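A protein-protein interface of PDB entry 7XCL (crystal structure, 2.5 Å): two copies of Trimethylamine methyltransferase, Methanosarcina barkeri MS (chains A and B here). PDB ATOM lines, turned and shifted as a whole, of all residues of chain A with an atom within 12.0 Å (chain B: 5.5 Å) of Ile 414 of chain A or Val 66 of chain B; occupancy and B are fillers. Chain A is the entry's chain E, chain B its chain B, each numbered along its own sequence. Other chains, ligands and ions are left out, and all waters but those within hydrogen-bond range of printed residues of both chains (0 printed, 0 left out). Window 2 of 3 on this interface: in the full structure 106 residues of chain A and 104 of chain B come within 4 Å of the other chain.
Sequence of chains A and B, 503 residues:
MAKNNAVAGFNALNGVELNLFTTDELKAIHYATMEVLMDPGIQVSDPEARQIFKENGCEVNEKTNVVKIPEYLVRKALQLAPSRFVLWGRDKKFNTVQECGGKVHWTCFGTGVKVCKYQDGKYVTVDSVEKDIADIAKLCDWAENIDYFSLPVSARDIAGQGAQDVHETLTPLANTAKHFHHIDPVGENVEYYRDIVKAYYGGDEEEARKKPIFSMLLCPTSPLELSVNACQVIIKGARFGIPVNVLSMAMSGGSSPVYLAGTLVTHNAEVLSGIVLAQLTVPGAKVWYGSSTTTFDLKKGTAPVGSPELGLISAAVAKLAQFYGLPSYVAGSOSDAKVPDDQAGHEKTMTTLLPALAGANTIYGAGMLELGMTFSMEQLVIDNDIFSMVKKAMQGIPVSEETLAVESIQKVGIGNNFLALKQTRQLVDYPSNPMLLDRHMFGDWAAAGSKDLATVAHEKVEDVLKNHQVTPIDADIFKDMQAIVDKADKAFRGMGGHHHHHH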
ATOM      1  N   ALA A 405      -5.880 -12.122   1.116  1.00  0.00           N
ATOM      2  CA  ALA A 405      -6.810 -12.840   1.979  1.00  0.00           C
ATOM      3  C   ALA A 405      -6.309 -14.107   2.674  1.00  0.00           C
ATOM      4  O   ALA A 405      -6.995 -15.141   2.679  1.00  0.00           O
ATOM      5  CB  ALA A 405      -8.074 -13.159   1.180  1.00  0.00           C
ATOM      6  N   VAL A 406      -5.134 -14.030   3.288  1.00  0.00           N
ATOM      7  CA  VAL A 406      -4.595 -15.193   3.978  1.00  0.00           C
ATOM      8  C   VAL A 406      -5.500 -15.674   5.117  1.00  0.00           C
ATOM      9  O   VAL A 406      -5.761 -16.872   5.244  1.00  0.00           O
ATOM     10  CB  VAL A 406      -3.187 -14.905   4.522  1.00  0.00           C
ATOM     11  CG1 VAL A 406      -2.728 -16.052   5.404  1.00  0.00           C
ATOM     12  CG2 VAL A 406      -2.215 -14.712   3.354  1.00  0.00           C
ATOM     13  N   GLU A 407      -5.992 -14.750   5.939  1.00  0.00           N
ATOM     14  CA  GLU A 407      -6.862 -15.133   7.045  1.00  0.00           C
ATOM     15  C   GLU A 407      -8.060 -15.927   6.549  1.00  0.00           C
ATOM     16  O   GLU A 407      -8.522 -16.846   7.227  1.00  0.00           O
ATOM     17  CB  GLU A 407      -7.319 -13.900   7.814  1.00  0.00           C
ATOM     18  CG  GLU A 407      -6.205 -13.267   8.628  1.00  0.00           C
ATOM     19  CD  GLU A 407      -6.595 -11.932   9.234  1.00  0.00           C
ATOM     20  OE1 GLU A 407      -5.745 -11.323   9.923  1.00  0.00           O
ATOM     21  OE2 GLU A 407      -7.745 -11.488   9.020  1.00  0.00           O
ATOM     22  N   SER A 408      -8.558 -15.581   5.365  1.00  0.00           N
ATOM     23  CA  SER A 408      -9.685 -16.299   4.783  1.00  0.00           C
ATOM     24  C   SER A 408      -9.272 -17.731   4.457  1.00  0.00           C
ATOM     25  O   SER A 408      -9.983 -18.683   4.776  1.00  0.00           O
ATOM     26  CB  SER A 408     -10.159 -15.620   3.500  1.00  0.00           C
ATOM     27  OG  SER A 408     -10.641 -14.322   3.772  1.00  0.00           O
ATOM     28  N   ILE A 409      -8.119 -17.880   3.811  1.00  0.00           N
ATOM     29  CA  ILE A 409      -7.634 -19.200   3.448  1.00  0.00           C
ATOM     30  C   ILE A 409      -7.455 -20.048   4.700  1.00  0.00           C
ATOM     31  O   ILE A 409      -7.783 -21.236   4.715  1.00  0.00           O
ATOM     32  CB  ILE A 409      -6.286 -19.123   2.715  1.00  0.00           C
ATOM     33  CG1 ILE A 409      -6.437 -18.276   1.450  1.00  0.00           C
ATOM     34  CG2 ILE A 409      -5.808 -20.534   2.376  1.00  0.00           C
ATOM     35  CD1 ILE A 409      -5.124 -17.994   0.739  1.00  0.00           C
ATOM     36  N   GLN A 410      -6.928 -19.434   5.751  1.00  0.00           N
ATOM     37  CA  GLN A 410      -6.713 -20.148   7.001  1.00  0.00           C
ATOM     38  C   GLN A 410      -8.024 -20.490   7.704  1.00  0.00           C
ATOM     39  O   GLN A 410      -8.163 -21.580   8.259  1.00  0.00           O
ATOM     40  CB  GLN A 410      -5.821 -19.332   7.917  1.00  0.00           C
ATOM     41  CG  GLN A 410      -4.364 -19.366   7.525  1.00  0.00           C
ATOM     42  CD  GLN A 410      -3.569 -18.291   8.239  1.00  0.00           C
ATOM     43  OE1 GLN A 410      -2.335 -18.303   8.245  1.00  0.00           O
ATOM     44  NE2 GLN A 410      -4.277 -17.343   8.841  1.00  0.00           N
ATOM     45  N   LYS A 411      -8.986 -19.576   7.672  1.00  0.00           N
ATOM     46  CA  LYS A 411     -10.262 -19.840   8.313  1.00  0.00           C
ATOM     47  C   LYS A 411     -11.005 -20.963   7.587  1.00  0.00           C
ATOM     48  O   LYS A 411     -11.478 -21.903   8.226  1.00  0.00           O
ATOM     49  CB  LYS A 411     -11.130 -18.581   8.353  1.00  0.00           C
ATOM     50  CG  LYS A 411     -12.364 -18.762   9.221  1.00  0.00           C
ATOM     51  CD  LYS A 411     -13.223 -17.514   9.305  1.00  0.00           C
ATOM     52  CE  LYS A 411     -14.431 -17.763  10.202  1.00  0.00           C
ATOM     53  NZ  LYS A 411     -15.355 -16.594  10.241  1.00  0.00           N
ATOM     54  N   VAL A 412     -11.113 -20.877   6.262  1.00  0.00           N
ATOM     55  CA  VAL A 412     -11.791 -21.929   5.514  1.00  0.00           C
ATOM     56  C   VAL A 412     -11.011 -23.232   5.709  1.00  0.00           C
ATOM     57  O   VAL A 412     -11.597 -24.306   5.857  1.00  0.00           O
ATOM     58  CB  VAL A 412     -11.887 -21.602   4.004  1.00  0.00           C
ATOM     59  CG1 VAL A 412     -12.564 -22.755   3.263  1.00  0.00           C
ATOM     60  CG2 VAL A 412     -12.684 -20.321   3.793  1.00  0.00           C
ATOM     61  N   GLY A 413      -9.686 -23.124   5.716  1.00  0.00           N
ATOM     62  CA  GLY A 413      -8.840 -24.286   5.925  1.00  0.00           C
ATOM     63  C   GLY A 413      -8.827 -25.357   4.853  1.00  0.00           C
ATOM     64  O   GLY A 413      -9.484 -25.248   3.817  1.00  0.00           O
ATOM     65  N   ILE A 414      -8.078 -26.417   5.134  1.00  0.00           N
ATOM     66  CA  ILE A 414      -7.920 -27.545   4.228  1.00  0.00           C
ATOM     67  C   ILE A 414      -9.210 -28.274   3.877  1.00  0.00           C
ATOM     68  O   ILE A 414     -10.024 -28.575   4.745  1.00  0.00           O
ATOM     69  CB  ILE A 414      -6.925 -28.585   4.821  1.00  0.00           C
ATOM     70  CG1 ILE A 414      -5.567 -27.928   5.060  1.00  0.00           C
ATOM     71  CG2 ILE A 414      -6.785 -29.781   3.885  1.00  0.00           C
ATOM     72  CD1 ILE A 414      -4.533 -28.840   5.694  1.00  0.00           C
ATOM     73  N   GLY A 415      -9.380 -28.549   2.586  1.00  0.00           N
ATOM     74  CA  GLY A 415     -10.531 -29.292   2.101  1.00  0.00           C
ATOM     75  C   GLY A 415     -11.938 -28.743   2.235  1.00  0.00           C
ATOM     76  O   GLY A 415     -12.898 -29.493   2.052  1.00  0.00           O
ATOM     77  N   ASN A 416     -12.085 -27.457   2.536  1.00  0.00           N
ATOM     78  CA  ASN A 416     -13.422 -26.880   2.672  1.00  0.00           C
ATOM     79  C   ASN A 416     -13.758 -25.902   1.554  1.00  0.00           C
ATOM     80  O   ASN A 416     -12.998 -25.781   0.595  1.00  0.00           O
ATOM     81  CB  ASN A 416     -13.549 -26.213   4.034  1.00  0.00           C
ATOM     82  CG  ASN A 416     -13.410 -27.209   5.160  1.00  0.00           C
ATOM     83  OD1 ASN A 416     -14.091 -28.236   5.171  1.00  0.00           O
ATOM     84  ND2 ASN A 416     -12.530 -26.920   6.108  1.00  0.00           N
ATOM     85  N   ASN A 417     -14.894 -25.217   1.647  1.00  0.00           N
ATOM     86  CA  ASN A 417     -15.235 -24.285   0.588  1.00  0.00           C
ATOM     87  C   ASN A 417     -15.634 -22.897   1.064  1.00  0.00           C
ATOM     88  O   ASN A 417     -16.060 -22.711   2.204  1.00  0.00           O
ATOM     89  CB  ASN A 417     -16.305 -24.887  -0.331  1.00  0.00           C
ATOM     90  CG  ASN A 417     -17.689 -24.770   0.224  1.00  0.00           C
ATOM     91  OD1 ASN A 417     -18.287 -23.695   0.211  1.00  0.00           O
ATOM     92  ND2 ASN A 417     -18.217 -25.879   0.719  1.00  0.00           N
ATOM     93  N   PHE A 418     -15.470 -21.927   0.165  1.00  0.00           N
ATOM     94  CA  PHE A 418     -15.739 -20.514   0.421  1.00  0.00           C
ATOM     95  C   PHE A 418     -17.150 -20.019   0.118  1.00  0.00           C
ATOM     96  O   PHE A 418     -17.462 -18.860   0.382  1.00  0.00           O
ATOM     97  CB  PHE A 418     -14.759 -19.656  -0.390  1.00  0.00           C
ATOM     98  CG  PHE A 418     -13.339 -19.735   0.081  1.00  0.00           C
ATOM     99  CD1 PHE A 418     -12.655 -20.950   0.085  1.00  0.00           C
ATOM    100  CD2 PHE A 418     -12.679 -18.589   0.520  1.00  0.00           C
ATOM    101  CE1 PHE A 418     -11.332 -21.024   0.522  1.00  0.00           C
ATOM    102  CE2 PHE A 418     -11.357 -18.650   0.959  1.00  0.00           C
ATOM    103  CZ  PHE A 418     -10.682 -19.874   0.960  1.00  0.00           C
ATOM    104  N   LEU A 421     -18.717 -18.412   3.240  1.00  0.00           N
ATOM    105  CA  LEU A 421     -17.952 -17.379   3.950  1.00  0.00           C
ATOM    106  C   LEU A 421     -18.618 -16.015   3.781  1.00  0.00           C
ATOM    107  O   LEU A 421     -19.155 -15.712   2.715  1.00  0.00           O
ATOM    108  CB  LEU A 421     -16.521 -17.340   3.408  1.00  0.00           C
ATOM    109  CG  LEU A 421     -15.446 -16.610   4.211  1.00  0.00           C
ATOM    110  CD1 LEU A 421     -15.267 -17.291   5.554  1.00  0.00           C
ATOM    111  CD2 LEU A 421     -14.139 -16.624   3.433  1.00  0.00           C
ATOM    112  N   PRO B  40      -2.582 -23.530   7.237  1.00  0.00           N
ATOM    113  CA  PRO B  40      -2.749 -24.890   7.762  1.00  0.00           C
ATOM    114  C   PRO B  40      -1.774 -25.928   7.248  1.00  0.00           C
ATOM    115  O   PRO B  40      -1.655 -27.011   7.817  1.00  0.00           O
ATOM    116  CB  PRO B  40      -4.166 -25.231   7.342  1.00  0.00           C
ATOM    117  CG  PRO B  40      -4.210 -24.628   5.973  1.00  0.00           C
ATOM    118  CD  PRO B  40      -3.604 -23.248   6.215  1.00  0.00           C
ATOM    119  N   GLY B  41      -1.083 -25.610   6.168  1.00  0.00           N
ATOM    120  CA  GLY B  41      -0.173 -26.580   5.603  1.00  0.00           C
ATOM    121  C   GLY B  41      -0.954 -27.338   4.546  1.00  0.00           C
ATOM    122  O   GLY B  41      -2.023 -26.888   4.102  1.00  0.00           O
ATOM    123  N   ILE B  42      -0.444 -28.502   4.158  1.00  0.00           N
ATOM    124  CA  ILE B  42      -1.085 -29.297   3.123  1.00  0.00           C
ATOM    125  C   ILE B  42      -1.326 -30.749   3.507  1.00  0.00           C
ATOM    126  O   ILE B  42      -0.447 -31.425   4.039  1.00  0.00           O
ATOM    127  CB  ILE B  42      -0.250 -29.221   1.817  1.00  0.00           C
ATOM    128  CG1 ILE B  42      -0.312 -27.781   1.289  1.00  0.00           C
ATOM    129  CG2 ILE B  42      -0.754 -30.240   0.782  1.00  0.00           C
ATOM    130  CD1 ILE B  42       0.424 -27.551   0.023  1.00  0.00           C
ATOM    131  N   GLN B  43      -2.534 -31.218   3.231  1.00  0.00           N
ATOM    132  CA  GLN B  43      -2.901 -32.589   3.531  1.00  0.00           C
ATOM    133  C   GLN B  43      -2.407 -33.536   2.440  1.00  0.00           C
ATOM    134  O   GLN B  43      -2.888 -33.498   1.310  1.00  0.00           O
ATOM    135  CB  GLN B  43      -4.415 -32.701   3.675  1.00  0.00           C
ATOM    136  CG  GLN B  43      -4.911 -34.114   3.853  1.00  0.00           C
ATOM    137  CD  GLN B  43      -6.400 -34.164   4.080  1.00  0.00           C
ATOM    138  OE1 GLN B  43      -6.894 -33.784   5.147  1.00  0.00           O
ATOM    139  NE2 GLN B  43      -7.132 -34.622   3.071  1.00  0.00           N
ATOM    140  N   VAL B  44      -1.441 -34.376   2.802  1.00  0.00           N
ATOM    141  CA  VAL B  44      -0.837 -35.353   1.900  1.00  0.00           C
ATOM    142  C   VAL B  44      -1.429 -36.733   2.212  1.00  0.00           C
ATOM    143  O   VAL B  44      -1.072 -37.361   3.208  1.00  0.00           O
ATOM    144  CB  VAL B  44       0.699 -35.365   2.096  1.00  0.00           C
ATOM    145  CG1 VAL B  44       1.355 -36.399   1.189  1.00  0.00           C
ATOM    146  CG2 VAL B  44       1.254 -33.977   1.819  1.00  0.00           C
ATOM    147  N   GLU B  59       7.169 -31.130   9.111  1.00  0.00           N
ATOM    148  CA  GLU B  59       6.402 -31.555  10.277  1.00  0.00           C
ATOM    149  C   GLU B  59       5.230 -32.305   9.666  1.00  0.00           C
ATOM    150  O   GLU B  59       4.578 -31.794   8.754  1.00  0.00           O
ATOM    151  CB  GLU B  59       5.859 -30.359  11.048  1.00  0.00           C
ATOM    152  CG  GLU B  59       6.898 -29.465  11.680  1.00  0.00           C
ATOM    153  CD  GLU B  59       6.262 -28.246  12.319  1.00  0.00           C
ATOM    154  OE1 GLU B  59       5.314 -28.426  13.120  1.00  0.00           O
ATOM    155  OE2 GLU B  59       6.705 -27.114  12.018  1.00  0.00           O
ATOM    156  N   VAL B  60       4.955 -33.508  10.153  1.00  0.00           N
ATOM    157  CA  VAL B  60       3.866 -34.296   9.595  1.00  0.00           C
ATOM    158  C   VAL B  60       2.944 -34.835  10.667  1.00  0.00           C
ATOM    159  O   VAL B  60       3.350 -35.669  11.470  1.00  0.00           O
ATOM    160  CB  VAL B  60       4.402 -35.500   8.799  1.00  0.00           C
ATOM    161  CG1 VAL B  60       3.256 -36.192   8.075  1.00  0.00           C
ATOM    162  CG2 VAL B  60       5.471 -35.049   7.824  1.00  0.00           C
ATOM    163  N   ASN B  61       1.707 -34.353  10.689  1.00  0.00           N
ATOM    164  CA  ASN B  61       0.739 -34.846  11.659  1.00  0.00           C
ATOM    165  C   ASN B  61       0.216 -36.128  11.033  1.00  0.00           C
ATOM    166  O   ASN B  61      -0.621 -36.093  10.129  1.00  0.00           O
ATOM    167  CB  ASN B  61      -0.401 -33.854  11.838  1.00  0.00           C
ATOM    168  CG  ASN B  61      -1.402 -34.315  12.867  1.00  0.00           C
ATOM    169  OD1 ASN B  61      -1.862 -35.456  12.829  1.00  0.00           O
ATOM    170  ND2 ASN B  61      -1.752 -33.431  13.793  1.00  0.00           N
ATOM    171  N   THR B  64      -3.824 -36.595  10.930  1.00  0.00           N
ATOM    172  CA  THR B  64      -4.571 -35.736  10.014  1.00  0.00           C
ATOM    173  C   THR B  64      -3.979 -35.736   8.600  1.00  0.00           C
ATOM    174  O   THR B  64      -4.618 -35.266   7.655  1.00  0.00           O
ATOM    175  CB  THR B  64      -4.594 -34.276  10.508  1.00  0.00           C
ATOM    176  OG1 THR B  64      -3.266 -33.740  10.474  1.00  0.00           O
ATOM    177  CG2 THR B  64      -5.119 -34.198  11.926  1.00  0.00           C
ATOM    178  N   ASN B  65      -2.761 -36.259   8.465  1.00  0.00           N
ATOM    179  CA  ASN B  65      -2.064 -36.317   7.178  1.00  0.00           C
ATOM    180  C   ASN B  65      -1.586 -34.944   6.722  1.00  0.00           C
ATOM    181  O   ASN B  65      -1.189 -34.772   5.571  1.00  0.00           O
ATOM    182  CB  ASN B  65      -2.962 -36.906   6.083  1.00  0.00           C
ATOM    183  CG  ASN B  65      -3.155 -38.408   6.216  1.00  0.00           C
ATOM    184  OD1 ASN B  65      -2.533 -39.061   7.061  1.00  0.00           O
ATOM    185  ND2 ASN B  65      -4.019 -38.967   5.369  1.00  0.00           N
ATOM    186  N   VAL B  66      -1.619 -33.967   7.623  1.00  0.00           N
ATOM    187  CA  VAL B  66      -1.200 -32.617   7.279  1.00  0.00           C
ATOM    188  C   VAL B  66       0.309 -32.414   7.334  1.00  0.00           C
ATOM    189  O   VAL B  66       0.953 -32.644   8.361  1.00  0.00           O
ATOM    190  CB  VAL B  66      -1.878 -31.566   8.189  1.00  0.00           C
ATOM    191  CG1 VAL B  66      -1.304 -30.191   7.907  1.00  0.00           C
ATOM    192  CG2 VAL B  66      -3.382 -31.556   7.939  1.00  0.00           C
ATOM    193  N   VAL B  67       0.860 -31.978   6.207  1.00  0.00           N
ATOM    194  CA  VAL B  67       2.287 -31.728   6.094  1.00  0.00           C
ATOM    195  C   VAL B  67       2.524 -30.223   6.043  1.00  0.00           C
ATOM    196  O   VAL B  67       1.835 -29.509   5.327  1.00  0.00           O
ATOM    197  CB  VAL B  67       2.860 -32.377   4.808  1.00  0.00           C
ATOM    198  CG1 VAL B  67       4.350 -32.066   4.677  1.00  0.00           C
ATOM    199  CG2 VAL B  67       2.616 -33.886   4.835  1.00  0.00           C
ATOM    200  N   LYS B  68       3.480 -29.745   6.828  1.00  0.00           N
ATOM    201  CA  LYS B  68       3.808 -28.329   6.836  1.00  0.00           C
ATOM    202  C   LYS B  68       5.175 -28.179   6.186  1.00  0.00           C
ATOM    203  O   LYS B  68       6.193 -28.641   6.710  1.00  0.00           O
ATOM    204  CB  LYS B  68       3.815 -27.779   8.264  1.00  0.00           C
ATOM    205  CG  LYS B  68       2.445 -27.816   8.910  1.00  0.00           C
ATOM    206  CD  LYS B  68       2.415 -27.121  10.262  1.00  0.00           C
ATOM    207  CE  LYS B  68       1.000 -27.136  10.840  1.00  0.00           C
ATOM    208  NZ  LYS B  68       0.849 -26.209  11.998  1.00  0.00           N
ATOM    209  N   PRO B 223      -9.247 -27.024  -1.468  1.00  0.00           N
ATOM    210  CA  PRO B 223      -7.999 -26.319  -1.164  1.00  0.00           C
ATOM    211  C   PRO B 223      -6.984 -27.053  -0.291  1.00  0.00           C
ATOM    212  O   PRO B 223      -7.335 -27.670   0.718  1.00  0.00           O
ATOM    213  CB  PRO B 223      -8.492 -25.045  -0.485  1.00  0.00           C
ATOM    214  CG  PRO B 223      -9.636 -25.558   0.331  1.00  0.00           C
ATOM    215  CD  PRO B 223     -10.342 -26.543  -0.604  1.00  0.00           C
ATOM    216  N   LEU B 224      -5.725 -26.981  -0.709  1.00  0.00           N
ATOM    217  CA  LEU B 224      -4.597 -27.534   0.029  1.00  0.00           C
ATOM    218  C   LEU B 224      -4.458 -29.044   0.266  1.00  0.00           C
ATOM    219  O   LEU B 224      -3.997 -29.465   1.327  1.00  0.00           O
ATOM    220  CB  LEU B 224      -4.508 -26.789   1.369  1.00  0.00           C
ATOM    221  CG  LEU B 224      -4.703 -25.270   1.236  1.00  0.00           C
ATOM    222  CD1 LEU B 224      -4.732 -24.614   2.608  1.00  0.00           C
ATOM    223  CD2 LEU B 224      -3.586 -24.690   0.379  1.00  0.00           C
ATOM    224  N   GLU B 225      -4.820 -29.862  -0.715  1.00  0.00           N
ATOM    225  CA  GLU B 225      -4.687 -31.309  -0.563  1.00  0.00           C
ATOM    226  C   GLU B 225      -3.952 -31.965  -1.731  1.00  0.00           C
ATOM    227  O   GLU B 225      -4.121 -31.573  -2.886  1.00  0.00           O
ATOM    228  CB  GLU B 225      -6.054 -31.986  -0.462  1.00  0.00           C
ATOM    229  CG  GLU B 225      -6.969 -31.487   0.625  1.00  0.00           C
ATOM    230  CD  GLU B 225      -8.241 -32.319   0.714  1.00  0.00           C
ATOM    231  OE1 GLU B 225      -8.886 -32.537  -0.336  1.00  0.00           O
ATOM    232  OE2 GLU B 225      -8.597 -32.756   1.830  1.00  0.00           O
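The side-chain carboxylate (OE2) of Glu 225 of chain B is in hydrogen-bond range of the side-chain amide nitrogen (NE2) of Gln 43 of chain B, 2.7 Å away. N of Val 66 of chain B lies close to OG1 of Thr 64 of chain B. The side-chain amide nitrogen (ND2) of Asn 416 of chain A lies within hydrogen-bond range of the backbone carbonyl oxygen (O) of Val 412 of chain A. ND2 of Asn 416 of chain A sits at hydrogen-bond distance from O of Ile 414 of chain A (3.3 Å). N of Asn 61 of chain B is in hydrogen-bond range of O of Val 66 of chain B (3.0 Å). O of Leu 224 of chain B lies within hydrogen-bond range of N of Gln 43 of chain B, 3.0 Å away.
The backbone NH (N) of Gly 415 of chain A sits at hydrogen-bond distance from the backbone carbonyl oxygen (O) of Pro 223 of chain B (2.9 Å).
Gly 413 of chain A touches Pro 223 of chain B. CG of Pro 40 of chain B touches CG1 of Ile 414 of chain A, 3.7 Å away. Ile 414 of chain A touches Gly 41 of chain B (CD1 to O, 3.6 Å). Ile 414 of chain A touches Gln 43 of chain B. CD1 of Ile 414 of chain A touches CG2 of Val 66 of chain B (3.7 Å). Pro 223 of chain B touches Ile 414 of chain A. Leu 224 of chain B touches Ile 414 of chain A. CG of Glu 225 of chain B touches CG2 of Ile 414 of chain A, at 3.7 Å. Gly 415 of chain A touches Glu 225 of chain B (CA to OE2, 3.98 Å). Asn 416 of chain A touches Pro 223 of chain B.
Of the 16 printed residues of chain B, 7 touch a printed residue of chain A. Hydrophobic or aromatic side chains of chain B within 4 Å of the printed part of chain A: Pro 40, Val 66 and Pro 223. Hydrophobic or aromatic side chains of chain A within 4 Å of the printed part of chain B: Ile 414. Along chain A the printed residues that touch a printed residue of chain B span positions 413 to 416. Among the printed residues, 11 pairs touch across the chains. Among the printed residues, no Asp or Glu carboxylate lies within 4 Å of a Lys or Arg side-chain nitrogen of the other chain.
Ala 405 of chain A touches none of the printed residues of chain B. Of the printed residues of chain B, Gly 413 of chain A touches Pro 223 (3.5 Å). Of the printed residues of chain B, Ile 414 of chain A touches Pro 40, Gly 41, Gln 43, Val 66, Pro 223, Leu 224 and Glu 225. Of the printed residues of chain B, Asn 416 of chain A touches Pro 223 (3.0 Å). Gly 41 of chain B touches just one residue of chain A: Ile 414 (3.6 Å). No residue of chain A comes within 4 Å of Ile 42 of chain B. No residue of chain A comes within 4 Å of Val 44 of chain B. No residue of chain A comes within 4 Å of Val 60 of chain B. No residue of chain A comes within 4 Å of Asn 61 of chain B. No residue of chain A comes within 4 Å of Asn 65 of chain B. Of chain A, only Ile 414 comes within 4 Å of Val 66 of chain B. No residue of chain A comes within 4 Å of Val 67 of chain B. No residue of chain A comes within 4 Å of Lys 68 of chain B. Pro 223 of chain B touches four residues of chain A. The nearest residue of chain B that does not touch Ile 414 of chain A is Ile 42 of chain B (4.3 Å). The nearest residue of chain A that does not touch Val 66 of chain B is Gly 415 of chain A (8.6 Å).
No position is printed for both chains.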
